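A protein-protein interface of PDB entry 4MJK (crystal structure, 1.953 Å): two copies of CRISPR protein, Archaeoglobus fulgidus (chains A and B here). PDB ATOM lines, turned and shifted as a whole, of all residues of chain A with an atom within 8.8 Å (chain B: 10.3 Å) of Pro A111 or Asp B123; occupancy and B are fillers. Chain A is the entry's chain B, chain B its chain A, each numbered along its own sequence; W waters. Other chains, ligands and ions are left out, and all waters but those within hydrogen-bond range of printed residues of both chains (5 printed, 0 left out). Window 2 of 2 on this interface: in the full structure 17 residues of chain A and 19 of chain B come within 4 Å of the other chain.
The backbone carbonyl oxygen (O) of Asn B122 lies within hydrogen-bond range of the side-chain hydroxyl (OG) of Ser B120 (2.9 Å). The backbone NH of Glu B124 is in hydrogen-bond range of the side-chain amide oxygen of Asn B122 (3.0 Å). O of Tyr A81 sits close to ND2 of Asn A85 (3.2 Å). The backbone carbonyl oxygen of Lys A115 lies within hydrogen-bond range of the backbone NH of Tyr A81 (3.0 Å). OE1 of Glu A154 sits at hydrogen-bond distance from OG of Ser A152 (3.4 Å). NZ of Lys A153 is in salt-bridge range of OE2 of Glu A154 (2.8 Å).
Among the printed residues, merely in contact across the chains: Glu A154 with Val B11, Pro A111 with Asn B122, Pro A111 with Asp B123 and Pro A111 with Leu B121.
No position is printed for both chains.
Of the 19 printed residues of chain A, 3 touch a printed residue of chain B. Hydrophobic or aromatic side chains of chain A that line the printed part of chain B: Tyr A81 and Pro A111. Hydrophobic or aromatic side chains of chain B within 4 Å of the printed part of chain A: Val B11. Along chain B the printed residues that touch a printed residue of chain A span positions 11 to 123. Among the printed residues, no Asp or Glu carboxylate lies within 4 Å of a Lys or Arg side-chain nitrogen of the other chain.
Water W3 lies within hydrogen-bond range of OD2 of Asp B123, NE of Arg A17 and O of Pro A111. Water W4 lies within hydrogen-bond range of O of Leu B121 (2.7 Å) and O of Ser A107 (3.1 Å). Water W1 bridges the backbone carbonyl oxygen of Ser B120 (2.8 Å) and the side-chain amino group of Lys A115 (2.9 Å). Water W2 lies within hydrogen-bond range of the backbone NH (N) of Ser B120 (3.1 Å), the side-chain amino group (NZ) of Lys A115 (3.1 Å) and the backbone carbonyl oxygen (O) of Leu B118 (3.3 Å). Water W5 lies within hydrogen-bond range of NZ of Lys A115 and O of Leu B118.
The side-chain hydroxyl of Ser B119 sits at hydrogen-bond distance from the side-chain hydroxyl of Tyr A81, at 2.6 Å.
Of the printed residues of chain B, Tyr A81 touches Ser B119 (2.6 Å). Lys A106 touches none of the printed residues of chain B. No residue of chain B comes within 4 Å of Ser A110. Of chain B, only Leu B121 (3.98 Å), Asn B122 (3.4 Å) and Asp B123 (3.6 Å) come within 4 Å of Pro A111. Printed residues of chain B within 4 Å of Glu A154: Val B11. Of the printed residues of chain A, Val B11 touches Glu A154. Of the printed residues of chain A, Ser B119 touches Tyr A81 (2.6 Å). Ala B125 touches none of the printed residues of chain A. The nearest residue of chain B that does not touch Pro A111 is Ser B120 (4.2 Å). The nearest printed residue of chain A that does not touch Ser B119 is Lys A115 (4.7 Å).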
ATOM      1  N   GLN A  15      27.688   7.618   6.529  1.00  0.00           N
ATOM      2  CA  GLN A  15      27.774   8.364   5.286  1.00  0.00           C
ATOM      3  C   GLN A  15      29.215   8.765   5.040  1.00  0.00           C
ATOM      4  O   GLN A  15      29.887   9.301   5.933  1.00  0.00           O
ATOM      5  CB  GLN A  15      26.875   9.604   5.301  1.00  0.00           C
ATOM      6  CG  GLN A  15      27.013  10.451   4.047  1.00  0.00           C
ATOM      7  CD  GLN A  15      25.887  11.460   3.893  1.00  0.00           C
ATOM      8  OE1 GLN A  15      25.245  11.846   4.873  1.00  0.00           O
ATOM      9  NE2 GLN A  15      25.628  11.870   2.658  1.00  0.00           N
ATOM     10  N   ALA A  16      29.701   8.457   3.844  1.00  0.00           N
ATOM     11  CA  ALA A  16      31.053   8.841   3.459  1.00  0.00           C
ATOM     12  C   ALA A  16      30.964   9.592   2.140  1.00  0.00           C
ATOM     13  O   ALA A  16      30.860   8.983   1.061  1.00  0.00           O
ATOM     14  CB  ALA A  16      31.939   7.624   3.335  1.00  0.00           C
ATOM     15  N   ARG A  17      30.970  10.917   2.231  1.00  0.00           N
ATOM     16  CA  ARG A  17      30.777  11.768   1.056  1.00  0.00           C
ATOM     17  C   ARG A  17      31.881  11.684  -0.006  1.00  0.00           C
ATOM     18  O   ARG A  17      31.671  12.093  -1.159  1.00  0.00           O
ATOM     19  CB  ARG A  17      30.516  13.219   1.481  1.00  0.00           C
ATOM     20  CG  ARG A  17      29.147  13.398   2.160  1.00  0.00           C
ATOM     21  CD  ARG A  17      28.960  14.819   2.625  1.00  0.00           C
ATOM     22  NE  ARG A  17      27.692  15.016   3.320  1.00  0.00           N
ATOM     23  CZ  ARG A  17      27.561  14.998   4.638  1.00  0.00           C
ATOM     24  NH1 ARG A  17      28.621  14.782   5.412  1.00  0.00           N
ATOM     25  NH2 ARG A  17      26.370  15.193   5.184  1.00  0.00           N
ATOM     26  N   TYR A  81      21.640   3.977   0.058  1.00  0.00           N
ATOM     27  CA  TYR A  81      20.552   4.913  -0.210  1.00  0.00           C
ATOM     28  C   TYR A  81      20.239   5.037  -1.693  1.00  0.00           C
ATOM     29  O   TYR A  81      19.129   5.426  -2.066  1.00  0.00           O
ATOM     30  CB  TYR A  81      20.844   6.288   0.381  1.00  0.00           C
ATOM     31  CG  TYR A  81      20.113   6.535   1.681  1.00  0.00           C
ATOM     32  CD1 TYR A  81      20.647   6.115   2.892  1.00  0.00           C
ATOM     33  CD2 TYR A  81      18.881   7.196   1.699  1.00  0.00           C
ATOM     34  CE1 TYR A  81      19.978   6.350   4.089  1.00  0.00           C
ATOM     35  CE2 TYR A  81      18.215   7.430   2.888  1.00  0.00           C
ATOM     36  CZ  TYR A  81      18.770   7.009   4.076  1.00  0.00           C
ATOM     37  OH  TYR A  81      18.111   7.240   5.263  1.00  0.00           O
ATOM     38  N   ASN A  85      16.389   4.998  -2.670  1.00  0.00           N
ATOM     39  CA  ASN A  85      15.891   6.186  -3.359  1.00  0.00           C
ATOM     40  C   ASN A  85      15.304   5.919  -4.743  1.00  0.00           C
ATOM     41  O   ASN A  85      14.348   6.592  -5.152  1.00  0.00           O
ATOM     42  CB  ASN A  85      16.974   7.271  -3.437  1.00  0.00           C
ATOM     43  CG  ASN A  85      17.188   7.971  -2.098  1.00  0.00           C
ATOM     44  OD1 ASN A  85      16.299   7.972  -1.252  1.00  0.00           O
ATOM     45  ND2 ASN A  85      18.355   8.563  -1.908  1.00  0.00           N
ATOM     46  N   ALA A 105      15.055  10.558  -8.171  1.00  0.00           N
ATOM     47  CA  ALA A 105      16.026   9.880  -7.326  1.00  0.00           C
ATOM     48  C   ALA A 105      17.325  10.682  -7.289  1.00  0.00           C
ATOM     49  O   ALA A 105      18.020  10.717  -6.273  1.00  0.00           O
ATOM     50  CB  ALA A 105      16.268   8.465  -7.825  1.00  0.00           C
ATOM     51  N   LYS A 106      17.641  11.337  -8.402  1.00  0.00           N
ATOM     52  CA  LYS A 106      18.811  12.207  -8.485  1.00  0.00           C
ATOM     53  C   LYS A 106      18.799  13.259  -7.374  1.00  0.00           C
ATOM     54  O   LYS A 106      19.834  13.543  -6.755  1.00  0.00           O
ATOM     55  CB  LYS A 106      18.850  12.892  -9.857  1.00  0.00           C
ATOM     56  CG  LYS A 106      19.952  13.920 -10.024  1.00  0.00           C
ATOM     57  CD  LYS A 106      20.396  14.014 -11.487  1.00  0.00           C
ATOM     58  CE  LYS A 106      19.833  15.244 -12.184  1.00  0.00           C
ATOM     59  NZ  LYS A 106      20.442  16.503 -11.664  1.00  0.00           N
ATOM     60  N   SER A 107      17.623  13.837  -7.137  1.00  0.00           N
ATOM     61  CA  SER A 107      17.448  14.852  -6.106  1.00  0.00           C
ATOM     62  C   SER A 107      17.618  14.271  -4.705  1.00  0.00           C
ATOM     63  O   SER A 107      18.198  14.904  -3.823  1.00  0.00           O
ATOM     64  CB  SER A 107      16.076  15.516  -6.238  1.00  0.00           C
ATOM     65  OG  SER A 107      16.110  16.571  -7.165  1.00  0.00           O
ATOM     66  N   PHE A 108      17.093  13.069  -4.508  1.00  0.00           N
ATOM     67  CA  PHE A 108      17.227  12.378  -3.235  1.00  0.00           C
ATOM     68  C   PHE A 108      18.673  11.965  -2.980  1.00  0.00           C
ATOM     69  O   PHE A 108      19.151  12.031  -1.844  1.00  0.00           O
ATOM     70  CB  PHE A 108      16.335  11.142  -3.202  1.00  0.00           C
ATOM     71  CG  PHE A 108      14.871  11.454  -3.173  1.00  0.00           C
ATOM     72  CD1 PHE A 108      14.424  12.728  -2.843  1.00  0.00           C
ATOM     73  CD2 PHE A 108      13.934  10.472  -3.474  1.00  0.00           C
ATOM     74  CE1 PHE A 108      13.078  13.015  -2.814  1.00  0.00           C
ATOM     75  CE2 PHE A 108      12.580  10.757  -3.448  1.00  0.00           C
ATOM     76  CZ  PHE A 108      12.153  12.028  -3.116  1.00  0.00           C
ATOM     77  N   ASP A 109      19.362  11.528  -4.033  1.00  0.00           N
ATOM     78  CA  ASP A 109      20.715  10.999  -3.900  1.00  0.00           C
ATOM     79  C   ASP A 109      21.744  12.090  -3.584  1.00  0.00           C
ATOM     80  O   ASP A 109      22.790  11.819  -2.991  1.00  0.00           O
ATOM     81  CB  ASP A 109      21.123  10.217  -5.162  1.00  0.00           C
ATOM     82  CG  ASP A 109      20.480   8.827  -5.238  1.00  0.00           C
ATOM     83  OD1 ASP A 109      20.021   8.312  -4.197  1.00  0.00           O
ATOM     84  OD2 ASP A 109      20.456   8.238  -6.342  1.00  0.00           O
ATOM     85  N   SER A 110      21.453  13.325  -3.967  1.00  0.00           N
ATOM     86  CA  SER A 110      22.434  14.391  -3.778  1.00  0.00           C
ATOM     87  C   SER A 110      22.888  14.568  -2.326  1.00  0.00           C
ATOM     88  O   SER A 110      24.082  14.477  -2.032  1.00  0.00           O
ATOM     89  CB  SER A 110      21.931  15.714  -4.358  1.00  0.00           C
ATOM     90  OG  SER A 110      23.030  16.422  -4.901  1.00  0.00           O
ATOM     91  N   PRO A 111      21.945  14.815  -1.407  1.00  0.00           N
ATOM     92  CA  PRO A 111      22.365  14.904  -0.004  1.00  0.00           C
ATOM     93  C   PRO A 111      22.745  13.542   0.592  1.00  0.00           C
ATOM     94  O   PRO A 111      23.307  13.497   1.689  1.00  0.00           O
ATOM     95  CB  PRO A 111      21.108  15.445   0.704  1.00  0.00           C
ATOM     96  CG  PRO A 111      19.966  14.952  -0.142  1.00  0.00           C
ATOM     97  CD  PRO A 111      20.494  15.028  -1.565  1.00  0.00           C
ATOM     98  N   ALA A 112      22.450  12.464  -0.130  1.00  0.00           N
ATOM     99  CA  ALA A 112      22.651  11.099   0.356  1.00  0.00           C
ATOM    100  C   ALA A 112      23.910  10.426  -0.216  1.00  0.00           C
ATOM    101  O   ALA A 112      24.058   9.200  -0.156  1.00  0.00           O
ATOM    102  CB  ALA A 112      21.407  10.244   0.040  1.00  0.00           C
ATOM    103  N   ARG A 113      24.809  11.222  -0.769  1.00  0.00           N
ATOM    104  CA  ARG A 113      25.996  10.682  -1.417  1.00  0.00           C
ATOM    105  C   ARG A 113      26.833   9.863  -0.423  1.00  0.00           C
ATOM    106  O   ARG A 113      27.222  10.365   0.626  1.00  0.00           O
ATOM    107  CB  ARG A 113      26.816  11.828  -2.028  1.00  0.00           C
ATOM    108  CG  ARG A 113      28.153  11.414  -2.582  1.00  0.00           C
ATOM    109  CD  ARG A 113      27.993  10.453  -3.760  1.00  0.00           C
ATOM    110  NE  ARG A 113      27.452  11.139  -4.930  1.00  0.00           N
ATOM    111  CZ  ARG A 113      27.273  10.566  -6.113  1.00  0.00           C
ATOM    112  NH1 ARG A 113      27.587   9.287  -6.284  1.00  0.00           N
ATOM    113  NH2 ARG A 113      26.778  11.272  -7.123  1.00  0.00           N
ATOM    114  N   GLY A 114      27.080   8.599  -0.739  1.00  0.00           N
ATOM    115  CA  GLY A 114      27.882   7.754   0.130  1.00  0.00           C
ATOM    116  C   GLY A 114      27.176   7.328   1.407  1.00  0.00           C
ATOM    117  O   GLY A 114      27.825   6.887   2.356  1.00  0.00           O
ATOM    118  N   LYS A 115      25.852   7.457   1.440  1.00  0.00           N
ATOM    119  CA  LYS A 115      25.093   7.102   2.642  1.00  0.00           C
ATOM    120  C   LYS A 115      24.445   5.736   2.540  1.00  0.00           C
ATOM    121  O   LYS A 115      23.825   5.405   1.522  1.00  0.00           O
ATOM    122  CB  LYS A 115      24.019   8.142   2.969  1.00  0.00           C
ATOM    123  CG  LYS A 115      23.243   7.792   4.236  1.00  0.00           C
ATOM    124  CD  LYS A 115      22.608   9.023   4.911  1.00  0.00           C
ATOM    125  CE  LYS A 115      21.542   9.658   4.044  1.00  0.00           C
ATOM    126  NZ  LYS A 115      20.753  10.724   4.784  1.00  0.00           N
ATOM    127  N   SER A 152      30.529  10.691   8.492  1.00  0.00           N
ATOM    128  CA  SER A 152      29.956  11.960   8.925  1.00  0.00           C
ATOM    129  C   SER A 152      29.775  11.977  10.439  1.00  0.00           C
ATOM    130  O   SER A 152      29.814  10.938  11.093  1.00  0.00           O
ATOM    131  CB  SER A 152      28.593  12.165   8.265  1.00  0.00           C
ATOM    132  OG  SER A 152      27.645  11.264   8.818  1.00  0.00           O
ATOM    133  N   LYS A 153      29.545  13.159  10.997  1.00  0.00           N
ATOM    134  CA  LYS A 153      29.373  13.263  12.435  1.00  0.00           C
ATOM    135  C   LYS A 153      28.117  12.538  12.918  1.00  0.00           C
ATOM    136  O   LYS A 153      28.045  12.126  14.081  1.00  0.00           O
ATOM    137  CB  LYS A 153      29.349  14.729  12.864  1.00  0.00           C
ATOM    138  CG  LYS A 153      28.257  15.545  12.236  1.00  0.00           C
ATOM    139  CD  LYS A 153      28.389  17.013  12.672  1.00  0.00           C
ATOM    140  CE  LYS A 153      27.104  17.792  12.411  1.00  0.00           C
ATOM    141  NZ  LYS A 153      25.972  17.212  13.198  1.00  0.00           N
ATOM    142  N   GLU A 154      27.136  12.374  12.030  1.00  0.00           N
ATOM    143  CA  GLU A 154      25.922  11.608  12.361  1.00  0.00           C
ATOM    144  C   GLU A 154      26.090  10.065  12.272  1.00  0.00           C
ATOM    145  O   GLU A 154      25.221   9.321  12.733  1.00  0.00           O
ATOM    146  CB  GLU A 154      24.736  12.062  11.502  1.00  0.00           C
ATOM    147  CG  GLU A 154      24.359  13.525  11.693  1.00  0.00           C
ATOM    148  CD  GLU A 154      25.182  14.476  10.810  1.00  0.00           C
ATOM    149  OE1 GLU A 154      25.929  13.994   9.922  1.00  0.00           O
ATOM    150  OE2 GLU A 154      25.080  15.711  11.003  1.00  0.00           O
ATOM    151  N   GLU B   9      16.138  19.163  16.016  1.00  0.00           N
ATOM    152  CA  GLU B   9      17.046  18.555  15.064  1.00  0.00           C
ATOM    153  C   GLU B   9      17.492  17.190  15.586  1.00  0.00           C
ATOM    154  O   GLU B   9      17.909  17.075  16.732  1.00  0.00           O
ATOM    155  CB  GLU B   9      18.247  19.488  14.890  1.00  0.00           C
ATOM    156  CG  GLU B   9      19.349  18.988  14.001  1.00  0.00           C
ATOM    157  CD  GLU B   9      20.502  19.989  13.948  1.00  0.00           C
ATOM    158  OE1 GLU B   9      21.601  19.654  14.437  1.00  0.00           O
ATOM    159  OE2 GLU B   9      20.289  21.115  13.444  1.00  0.00           O
ATOM    160  N   PHE B  10      17.393  16.160  14.755  1.00  0.00           N
ATOM    161  CA  PHE B  10      17.751  14.797  15.166  1.00  0.00           C
ATOM    162  C   PHE B  10      19.114  14.471  14.581  1.00  0.00           C
ATOM    163  O   PHE B  10      19.421  14.892  13.470  1.00  0.00           O
ATOM    164  CB  PHE B  10      16.713  13.761  14.656  1.00  0.00           C
ATOM    165  CG  PHE B  10      15.397  13.788  15.406  1.00  0.00           C
ATOM    166  CD1 PHE B  10      14.532  14.864  15.276  1.00  0.00           C
ATOM    167  CD2 PHE B  10      15.040  12.744  16.256  1.00  0.00           C
ATOM    168  CE1 PHE B  10      13.334  14.894  15.969  1.00  0.00           C
ATOM    169  CE2 PHE B  10      13.849  12.772  16.962  1.00  0.00           C
ATOM    170  CZ  PHE B  10      12.987  13.853  16.815  1.00  0.00           C
ATOM    171  N   VAL B  11      19.927  13.732  15.323  1.00  0.00           N
ATOM    172  CA  VAL B  11      21.175  13.204  14.782  1.00  0.00           C
ATOM    173  C   VAL B  11      20.899  12.213  13.648  1.00  0.00           C
ATOM    174  O   VAL B  11      21.510  12.319  12.580  1.00  0.00           O
ATOM    175  CB  VAL B  11      22.035  12.535  15.893  1.00  0.00           C
ATOM    176  CG1 VAL B  11      23.303  11.863  15.314  1.00  0.00           C
ATOM    177  CG2 VAL B  11      22.410  13.570  16.967  1.00  0.00           C
ATOM    178  N   LEU B  74      10.147  19.239   8.753  1.00  0.00           N
ATOM    179  CA  LEU B  74      10.541  20.463   8.074  1.00  0.00           C
ATOM    180  C   LEU B  74      11.396  20.150   6.857  1.00  0.00           C
ATOM    181  O   LEU B  74      11.375  20.883   5.874  1.00  0.00           O
ATOM    182  CB  LEU B  74      11.311  21.389   9.037  1.00  0.00           C
ATOM    183  CG  LEU B  74      10.496  21.781  10.284  1.00  0.00           C
ATOM    184  CD1 LEU B  74      11.316  22.584  11.299  1.00  0.00           C
ATOM    185  CD2 LEU B  74       9.254  22.543   9.872  1.00  0.00           C
ATOM    186  N   ASN B  75      12.145  19.057   6.904  1.00  0.00           N
ATOM    187  CA  ASN B  75      13.102  18.791   5.833  1.00  0.00           C
ATOM    188  C   ASN B  75      13.473  17.319   5.722  1.00  0.00           C
ATOM    189  O   ASN B  75      14.554  16.979   5.256  1.00  0.00           O
ATOM    190  CB  ASN B  75      14.387  19.583   6.083  1.00  0.00           C
ATOM    191  CG  ASN B  75      15.157  19.048   7.267  1.00  0.00           C
ATOM    192  OD1 ASN B  75      14.591  18.353   8.114  1.00  0.00           O
ATOM    193  ND2 ASN B  75      16.451  19.325   7.321  1.00  0.00           N
ATOM    194  N   CYS B  76      12.590  16.436   6.163  1.00  0.00           N
ATOM    195  CA  CYS B  76      12.970  15.034   6.234  1.00  0.00           C
ATOM    196  C   CYS B  76      11.784  14.114   6.008  1.00  0.00           C
ATOM    197  O   CYS B  76      10.618  14.538   6.032  1.00  0.00           O
ATOM    198  CB  CYS B  76      13.660  14.721   7.574  1.00  0.00           C
ATOM    199  SG  CYS B  76      12.608  14.908   9.050  1.00  0.00           S
ATOM    200  N   THR B  77      12.103  12.850   5.768  1.00  0.00           N
ATOM    201  CA  THR B  77      11.092  11.836   5.531  1.00  0.00           C
ATOM    202  C   THR B  77      11.511  10.588   6.341  1.00  0.00           C
ATOM    203  O   THR B  77      12.689  10.198   6.349  1.00  0.00           O
ATOM    204  CB  THR B  77      10.966  11.547   4.005  1.00  0.00           C
ATOM    205  OG1 THR B  77       9.730  10.862   3.722  1.00  0.00           O
ATOM    206  CG2 THR B  77      12.116  10.704   3.534  1.00  0.00           C
ATOM    207  N   LEU B 118      15.416   9.072  10.222  1.00  0.00           N
ATOM    208  CA  LEU B 118      14.851  10.267   9.590  1.00  0.00           C
ATOM    209  C   LEU B 118      15.818  10.714   8.520  1.00  0.00           C
ATOM    210  O   LEU B 118      16.946  11.103   8.817  1.00  0.00           O
ATOM    211  CB  LEU B 118      14.589  11.374  10.617  1.00  0.00           C
ATOM    212  CG  LEU B 118      13.486  11.053  11.638  1.00  0.00           C
ATOM    213  CD1 LEU B 118      13.477  12.062  12.792  1.00  0.00           C
ATOM    214  CD2 LEU B 118      12.086  10.989  10.964  1.00  0.00           C
ATOM    215  N   SER B 119      15.398  10.586   7.267  1.00  0.00           N
ATOM    216  CA  SER B 119      16.260  10.911   6.132  1.00  0.00           C
ATOM    217  C   SER B 119      16.054  12.364   5.713  1.00  0.00           C
ATOM    218  O   SER B 119      14.966  12.756   5.300  1.00  0.00           O
ATOM    219  CB  SER B 119      15.936  10.021   4.927  1.00  0.00           C
ATOM    220  OG  SER B 119      15.893   8.651   5.274  1.00  0.00           O
ATOM    221  N   SER B 120      17.101  13.160   5.802  1.00  0.00           N
ATOM    222  CA  SER B 120      17.011  14.539   5.383  1.00  0.00           C
ATOM    223  C   SER B 120      16.883  14.656   3.865  1.00  0.00           C
ATOM    224  O   SER B 120      17.493  13.891   3.104  1.00  0.00           O
ATOM    225  CB  SER B 120      18.226  15.318   5.864  1.00  0.00           C
ATOM    226  OG  SER B 120      18.103  16.677   5.487  1.00  0.00           O
ATOM    227  N   LEU B 121      16.090  15.629   3.432  1.00  0.00           N
ATOM    228  CA  LEU B 121      15.911  15.915   2.015  1.00  0.00           C
ATOM    229  C   LEU B 121      16.852  17.024   1.545  1.00  0.00           C
ATOM    230  O   LEU B 121      16.859  17.380   0.370  1.00  0.00           O
ATOM    231  CB  LEU B 121      14.458  16.313   1.732  1.00  0.00           C
ATOM    232  CG  LEU B 121      13.480  15.190   2.070  1.00  0.00           C
ATOM    233  CD1 LEU B 121      12.029  15.667   2.005  1.00  0.00           C
ATOM    234  CD2 LEU B 121      13.724  13.981   1.165  1.00  0.00           C
ATOM    235  N   ASN B 122      17.630  17.581   2.458  1.00  0.00           N
ATOM    236  CA  ASN B 122      18.645  18.554   2.070  1.00  0.00           C
ATOM    237  C   ASN B 122      19.919  18.273   2.858  1.00  0.00           C
ATOM    238  O   ASN B 122      20.050  17.202   3.447  1.00  0.00           O
ATOM    239  CB  ASN B 122      18.142  19.999   2.246  1.00  0.00           C
ATOM    240  CG  ASN B 122      17.840  20.349   3.695  1.00  0.00           C
ATOM    241  OD1 ASN B 122      18.122  19.575   4.608  1.00  0.00           O
ATOM    242  ND2 ASN B 122      17.264  21.528   3.910  1.00  0.00           N
ATOM    243  N   ASP B 123      20.863  19.207   2.887  1.00  0.00           N
ATOM    244  CA  ASP B 123      22.138  18.900   3.541  1.00  0.00           C
ATOM    245  C   ASP B 123      22.121  19.161   5.040  1.00  0.00           C
ATOM    246  O   ASP B 123      23.140  19.020   5.709  1.00  0.00           O
ATOM    247  CB  ASP B 123      23.320  19.632   2.882  1.00  0.00           C
ATOM    248  CG  ASP B 123      23.987  18.803   1.789  1.00  0.00           C
ATOM    249  OD1 ASP B 123      23.281  18.355   0.861  1.00  0.00           O
ATOM    250  OD2 ASP B 123      25.223  18.593   1.860  1.00  0.00           O
ATOM    251  N   GLU B 124      20.968  19.531   5.579  1.00  0.00           N
ATOM    252  CA  GLU B 124      20.887  19.749   7.023  1.00  0.00           C
ATOM    253  C   GLU B 124      20.512  18.473   7.752  1.00  0.00           C
ATOM    254  O   GLU B 124      19.996  17.525   7.156  1.00  0.00           O
ATOM    255  CB  GLU B 124      19.841  20.802   7.352  1.00  0.00           C
ATOM    256  CG  GLU B 124      20.002  22.113   6.631  1.00  0.00           C
ATOM    257  CD  GLU B 124      19.007  23.127   7.138  1.00  0.00           C
ATOM    258  OE1 GLU B 124      17.852  23.131   6.648  1.00  0.00           O
ATOM    259  OE2 GLU B 124      19.375  23.901   8.051  1.00  0.00           O
ATOM    260  N   ALA B 125      20.761  18.463   9.055  1.00  0.00           N
ATOM    261  CA  ALA B 125      20.282  17.392   9.912  1.00  0.00           C
ATOM    262  C   ALA B 125      18.745  17.374   9.839  1.00  0.00           C
ATOM    263  O   ALA B 125      18.117  18.399   9.616  1.00  0.00           O
ATOM    264  CB  ALA B 125      20.751  17.628  11.334  1.00  0.00           C
ATOM    265  N   PRO B 126      18.136  16.196   9.992  1.00  0.00           N
ATOM    266  CA  PRO B 126      16.670  16.139   9.886  1.00  0.00           C
ATOM    267  C   PRO B 126      15.984  16.850  11.059  1.00  0.00           C
ATOM    268  O   PRO B 126      16.400  16.680  12.208  1.00  0.00           O
ATOM    269  CB  PRO B 126      16.375  14.641   9.922  1.00  0.00           C
ATOM    270  CG  PRO B 126      17.576  14.028  10.563  1.00  0.00           C
ATOM    271  CD  PRO B 126      18.742  14.872  10.197  1.00  0.00           C
ATOM    272  N   LYS B 127      14.944  17.621  10.763  1.00  0.00           N
ATOM    273  CA  LYS B 127      14.257  18.418  11.764  1.00  0.00           C
ATOM    274  C   LYS B 127      12.749  18.186  11.752  1.00  0.00           C
ATOM    275  O   LYS B 127      12.150  18.023  10.693  1.00  0.00           O
ATOM    276  CB  LYS B 127      14.523  19.910  11.524  1.00  0.00           C
ATOM    277  CG  LYS B 127      15.941  20.345  11.872  1.00  0.00           C
ATOM    278  CD  LYS B 127      16.076  21.866  11.781  1.00  0.00           C
ATOM    279  CE  LYS B 127      15.823  22.349  10.360  1.00  0.00           C
ATOM    280  NZ  LYS B 127      15.555  23.826  10.296  1.00  0.00           N
ATOM    281  N   SER B 235       9.006  15.908  -0.776  1.00  0.00           N
ATOM    282  CA  SER B 235       9.908  16.835  -1.441  1.00  0.00           C
ATOM    283  C   SER B 235      10.214  17.965  -0.488  1.00  0.00           C
ATOM    284  O   SER B 235       9.354  18.375   0.304  1.00  0.00           O
ATOM    285  CB  SER B 235       9.258  17.393  -2.716  1.00  0.00           C
ATOM    286  OG  SER B 235       9.850  18.625  -3.118  1.00  0.00           O
ATOM    287  N   ILE B 236      11.436  18.479  -0.568  1.00  0.00           N
ATOM    288  CA  ILE B 236      11.848  19.585   0.285  1.00  0.00           C
ATOM    289  C   ILE B 236      10.942  20.803   0.081  1.00  0.00           C
ATOM    290  O   ILE B 236      10.826  21.655   0.960  1.00  0.00           O
ATOM    291  CB  ILE B 236      13.331  19.959   0.030  1.00  0.00           C
ATOM    292  CG1 ILE B 236      13.830  20.966   1.069  1.00  0.00           C
ATOM    293  CG2 ILE B 236      13.528  20.484  -1.402  1.00  0.00           C
ATOM    294  CD1 ILE B 236      13.834  20.431   2.490  1.00  0.00           C
HETATM  295  O   HOH W   1      18.871  11.490   2.670  1.00  0.00           O
HETATM  296  O   HOH W   2      19.641  12.175   7.324  1.00  0.00           O
HETATM  297  O   HOH W   3      25.072  16.014   2.353  1.00  0.00           O
HETATM  298  O   HOH W   4      16.057  15.779  -1.697  1.00  0.00           O
HETATM  299  O   HOH W   5      19.818   9.573   7.530  1.00  0.00           O
